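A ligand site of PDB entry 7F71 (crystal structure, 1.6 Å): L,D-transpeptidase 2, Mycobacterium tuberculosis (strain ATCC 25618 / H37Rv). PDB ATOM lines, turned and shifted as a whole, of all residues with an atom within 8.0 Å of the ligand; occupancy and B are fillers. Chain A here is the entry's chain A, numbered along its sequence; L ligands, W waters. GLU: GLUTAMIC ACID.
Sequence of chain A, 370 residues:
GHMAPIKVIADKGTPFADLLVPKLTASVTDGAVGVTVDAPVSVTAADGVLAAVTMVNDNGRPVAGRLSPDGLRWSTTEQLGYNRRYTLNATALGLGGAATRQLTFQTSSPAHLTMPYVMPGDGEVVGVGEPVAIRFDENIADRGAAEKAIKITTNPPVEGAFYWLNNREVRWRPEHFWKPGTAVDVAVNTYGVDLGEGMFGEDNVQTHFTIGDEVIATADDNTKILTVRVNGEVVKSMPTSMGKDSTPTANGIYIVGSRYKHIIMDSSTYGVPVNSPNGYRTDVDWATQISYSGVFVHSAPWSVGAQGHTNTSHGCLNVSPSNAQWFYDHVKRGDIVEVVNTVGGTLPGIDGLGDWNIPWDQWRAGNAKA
The side-chain amide nitrogen (ND2) of Asn 275 is in hydrogen-bond range of an oxygen (OXT) of the ligand (2.8 Å). The backbone NH (N) of Asn 275 sits at hydrogen-bond distance from an oxygen (O) of the ligand, at 2.7 Å. The backbone NH (N) of Val 274 is in hydrogen-bond range of an oxygen (O) of the ligand, 2.7 Å away.
The backbone carbonyl oxygen (O) of Pro 273 lies within hydrogen-bond range of the side-chain hydroxyl (OG) of Ser 276, at 2.7 Å. The side-chain carboxylate (OD1) of Asp 266 is in hydrogen-bond range of the side-chain hydroxyl (OG) of Ser 268, 2.5 Å away.
Ser 268 touches the ligand (CB to N, 3.3 Å). Pro 273 touches the ligand (CB to O, 2.9 Å). Within 4 Å of the ligand: Ser 268, Pro 273, Val 274 and Asn 275. The nearest printed residue that does not touch the ligand is Ser 276 (4.2 Å).
Water W2 lies within hydrogen-bond range of O of Ser 268 (2.7 Å), OE2 of the ligand (3.2 Å) and N of Gly 271 (3.5 Å).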
ATOM      1  N   ASP A 266      23.612  -9.662  15.389  1.00  0.00           N
ATOM      2  CA  ASP A 266      23.193 -10.448  14.230  1.00  0.00           C
ATOM      3  C   ASP A 266      24.296 -10.310  13.193  1.00  0.00           C
ATOM      4  O   ASP A 266      24.470  -9.230  12.638  1.00  0.00           O
ATOM      5  CB  ASP A 266      21.854  -9.931  13.708  1.00  0.00           C
ATOM      6  CG  ASP A 266      21.318 -10.730  12.538  1.00  0.00           C
ATOM      7  OD1 ASP A 266      22.134 -11.332  11.807  1.00  0.00           O
ATOM      8  OD2 ASP A 266      20.072 -10.755  12.353  1.00  0.00           O
ATOM      9  N   SER A 267      25.039 -11.382  12.957  1.00  0.00           N
ATOM     10  CA  SER A 267      26.194 -11.289  12.057  1.00  0.00           C
ATOM     11  C   SER A 267      25.797 -10.820  10.665  1.00  0.00           C
ATOM     12  O   SER A 267      26.624 -10.245   9.959  1.00  0.00           O
ATOM     13  CB  SER A 267      26.933 -12.626  11.956  1.00  0.00           C
ATOM     14  OG  SER A 267      26.096 -13.648  11.445  1.00  0.00           O
ATOM     15  N   SER A 268      24.537 -11.051  10.262  1.00  0.00           N
ATOM     16  CA  SER A 268      24.105 -10.577   8.946  1.00  0.00           C
ATOM     17  C   SER A 268      24.155  -9.061   8.864  1.00  0.00           C
ATOM     18  O   SER A 268      24.330  -8.496   7.778  1.00  0.00           O
ATOM     19  CB  SER A 268      22.697 -11.108   8.628  1.00  0.00           C
ATOM     20  OG  SER A 268      21.701 -10.608   9.501  1.00  0.00           O
ATOM     21  N   THR A 269      24.031  -8.381  10.011  1.00  0.00           N
ATOM     22  CA  THR A 269      24.228  -6.932  10.038  1.00  0.00           C
ATOM     23  C   THR A 269      25.631  -6.529   9.610  1.00  0.00           C
ATOM     24  O   THR A 269      25.826  -5.430   9.079  1.00  0.00           O
ATOM     25  CB  THR A 269      23.947  -6.406  11.454  1.00  0.00           C
ATOM     26  OG1 THR A 269      22.622  -6.800  11.847  1.00  0.00           O
ATOM     27  CG2 THR A 269      24.072  -4.891  11.514  1.00  0.00           C
ATOM     28  N   TYR A 270      26.617  -7.404   9.812  1.00  0.00           N
ATOM     29  CA  TYR A 270      28.019  -7.097   9.535  1.00  0.00           C
ATOM     30  C   TYR A 270      28.557  -7.913   8.362  1.00  0.00           C
ATOM     31  O   TYR A 270      29.766  -8.098   8.235  1.00  0.00           O
ATOM     32  CB  TYR A 270      28.857  -7.296  10.802  1.00  0.00           C
ATOM     33  CG  TYR A 270      28.171  -6.709  12.028  1.00  0.00           C
ATOM     34  CD1 TYR A 270      28.015  -5.325  12.170  1.00  0.00           C
ATOM     35  CD2 TYR A 270      27.626  -7.537  13.003  1.00  0.00           C
ATOM     36  CE1 TYR A 270      27.344  -4.785  13.274  1.00  0.00           C
ATOM     37  CE2 TYR A 270      26.962  -7.010  14.107  1.00  0.00           C
ATOM     38  CZ  TYR A 270      26.822  -5.633  14.236  1.00  0.00           C
ATOM     39  OH  TYR A 270      26.154  -5.116  15.332  1.00  0.00           O
ATOM     40  N   GLY A 271      27.670  -8.386   7.490  1.00  0.00           N
ATOM     41  CA  GLY A 271      28.070  -9.003   6.229  1.00  0.00           C
ATOM     42  C   GLY A 271      28.303 -10.507   6.259  1.00  0.00           C
ATOM     43  O   GLY A 271      28.859 -11.035   5.295  1.00  0.00           O
ATOM     44  N   VAL A 272      27.905 -11.203   7.318  1.00  0.00           N
ATOM     45  CA  VAL A 272      28.194 -12.608   7.493  1.00  0.00           C
ATOM     46  C   VAL A 272      26.873 -13.366   7.726  1.00  0.00           C
ATOM     47  O   VAL A 272      26.232 -13.129   8.760  1.00  0.00           O
ATOM     48  CB  VAL A 272      29.167 -12.888   8.648  1.00  0.00           C
ATOM     49  CG1 VAL A 272      29.329 -14.382   8.857  1.00  0.00           C
ATOM     50  CG2 VAL A 272      30.490 -12.216   8.404  1.00  0.00           C
ATOM     51  N   PRO A 273      26.468 -14.266   6.854  1.00  0.00           N
ATOM     52  CA  PRO A 273      25.200 -14.973   7.073  1.00  0.00           C
ATOM     53  C   PRO A 273      25.206 -15.739   8.385  1.00  0.00           C
ATOM     54  O   PRO A 273      26.193 -16.392   8.754  1.00  0.00           O
ATOM     55  CB  PRO A 273      25.101 -15.904   5.858  1.00  0.00           C
ATOM     56  CG  PRO A 273      25.905 -15.204   4.793  1.00  0.00           C
ATOM     57  CD  PRO A 273      27.052 -14.571   5.534  1.00  0.00           C
ATOM     58  N   VAL A 274      24.093 -15.635   9.114  1.00  0.00           N
ATOM     59  CA  VAL A 274      23.987 -16.292  10.415  1.00  0.00           C
ATOM     60  C   VAL A 274      24.280 -17.789  10.287  1.00  0.00           C
ATOM     61  O   VAL A 274      25.026 -18.361  11.094  1.00  0.00           O
ATOM     62  CB  VAL A 274      22.595 -16.037  11.019  1.00  0.00           C
ATOM     63  CG1 VAL A 274      22.422 -16.825  12.307  1.00  0.00           C
ATOM     64  CG2 VAL A 274      22.378 -14.533  11.240  1.00  0.00           C
ATOM     65  N   ASN A 275      23.690 -18.434   9.284  1.00  0.00           N
ATOM     66  CA  ASN A 275      23.803 -19.872   9.079  1.00  0.00           C
ATOM     67  C   ASN A 275      25.144 -20.289   8.468  1.00  0.00           C
ATOM     68  O   ASN A 275      25.323 -21.486   8.182  1.00  0.00           O
ATOM     69  CB  ASN A 275      22.660 -20.303   8.171  1.00  0.00           C
ATOM     70  CG  ASN A 275      21.283 -20.056   8.777  1.00  0.00           C
ATOM     71  OD1 ASN A 275      21.096 -20.038  10.005  1.00  0.00           O
ATOM     72  ND2 ASN A 275      20.300 -19.926   7.898  1.00  0.00           N
ATOM     73  N   SER A 276      26.080 -19.365   8.280  1.00  0.00           N
ATOM     74  CA  SER A 276      27.391 -19.670   7.716  1.00  0.00           C
ATOM     75  C   SER A 276      28.367 -20.052   8.815  1.00  0.00           C
ATOM     76  O   SER A 276      28.081 -19.902  10.006  1.00  0.00           O
ATOM     77  CB  SER A 276      27.904 -18.469   6.920  1.00  0.00           C
ATOM     78  OG  SER A 276      28.462 -17.465   7.761  1.00  0.00           O
ATOM     79  N   PRO A 277      29.548 -20.545   8.450  1.00  0.00           N
ATOM     80  CA  PRO A 277      30.451 -21.100   9.485  1.00  0.00           C
ATOM     81  C   PRO A 277      30.791 -20.107  10.597  1.00  0.00           C
ATOM     82  O   PRO A 277      30.894 -20.504  11.766  1.00  0.00           O
ATOM     83  CB  PRO A 277      31.686 -21.507   8.680  1.00  0.00           C
ATOM     84  CG  PRO A 277      31.193 -21.702   7.268  1.00  0.00           C
ATOM     85  CD  PRO A 277      30.109 -20.686   7.093  1.00  0.00           C
ATOM     86  N   GLY A 279      28.911 -17.309  11.265  1.00  0.00           N
ATOM     87  CA  GLY A 279      27.754 -16.508  11.599  1.00  0.00           C
ATOM     88  C   GLY A 279      27.239 -16.789  12.981  1.00  0.00           C
ATOM     89  O   GLY A 279      27.582 -17.792  13.629  1.00  0.00           O
ATOM     90  N   TYR A 280      26.399 -15.864  13.457  1.00  0.00           N
ATOM     91  CA  TYR A 280      25.843 -15.927  14.803  1.00  0.00           C
ATOM     92  C   TYR A 280      24.653 -14.983  14.886  1.00  0.00           C
ATOM     93  O   TYR A 280      24.560 -14.001  14.138  1.00  0.00           O
ATOM     94  CB  TYR A 280      26.882 -15.551  15.870  1.00  0.00           C
ATOM     95  CG  TYR A 280      27.544 -14.218  15.628  1.00  0.00           C
ATOM     96  CD1 TYR A 280      26.936 -13.030  16.038  1.00  0.00           C
ATOM     97  CD2 TYR A 280      28.754 -14.129  14.960  1.00  0.00           C
ATOM     98  CE1 TYR A 280      27.520 -11.809  15.805  1.00  0.00           C
ATOM     99  CE2 TYR A 280      29.360 -12.906  14.722  1.00  0.00           C
ATOM    100  CZ  TYR A 280      28.733 -11.751  15.150  1.00  0.00           C
ATOM    101  OH  TYR A 280      29.321 -10.537  14.910  1.00  0.00           O
ATOM    102  N   ARG A 281      23.739 -15.286  15.811  1.00  0.00           N
ATOM    103  CA  ARG A 281      22.665 -14.371  16.194  1.00  0.00           C
ATOM    104  C   ARG A 281      22.507 -14.602  17.689  1.00  0.00           C
ATOM    105  O   ARG A 281      21.949 -15.626  18.098  1.00  0.00           O
ATOM    106  CB  ARG A 281      21.353 -14.619  15.436  1.00  0.00           C
ATOM    107  CG  ARG A 281      20.302 -13.492  15.555  1.00  0.00           C
ATOM    108  CD  ARG A 281      19.059 -13.767  14.617  1.00  0.00           C
ATOM    109  NE  ARG A 281      18.999 -15.216  14.481  1.00  0.00           N
ATOM    110  CZ  ARG A 281      18.828 -15.898  13.358  1.00  0.00           C
ATOM    111  NH1 ARG A 281      18.594 -15.290  12.180  1.00  0.00           N
ATOM    112  NH2 ARG A 281      18.868 -17.216  13.437  1.00  0.00           N
HETATM  113  N   GLU L   1      21.863 -14.199   7.869  1.00  0.00           N
HETATM  114  CA  GLU L   1      21.327 -14.999   6.798  1.00  0.00           C
HETATM  115  C   GLU L   1      21.647 -16.482   7.058  1.00  0.00           C
HETATM  116  O   GLU L   1      22.766 -16.962   7.170  1.00  0.00           O
HETATM  117  CB  GLU L   1      21.872 -14.424   5.498  1.00  0.00           C
HETATM  118  CG  GLU L   1      21.827 -12.902   5.628  1.00  0.00           C
HETATM  119  CD  GLU L   1      22.415 -12.115   4.470  1.00  0.00           C
HETATM  120  OE1 GLU L   1      22.796 -12.702   3.430  1.00  0.00           O
HETATM  121  OE2 GLU L   1      22.466 -10.870   4.616  1.00  0.00           O
HETATM  122  OXT GLU L   1      20.728 -17.263   7.247  1.00  0.00           O
HETATM  123  O   HOH W   1      18.307 -16.736   7.396  1.00  0.00           O
HETATM  124  O   HOH W   2      25.071  -9.241   5.327  1.00  0.00           O
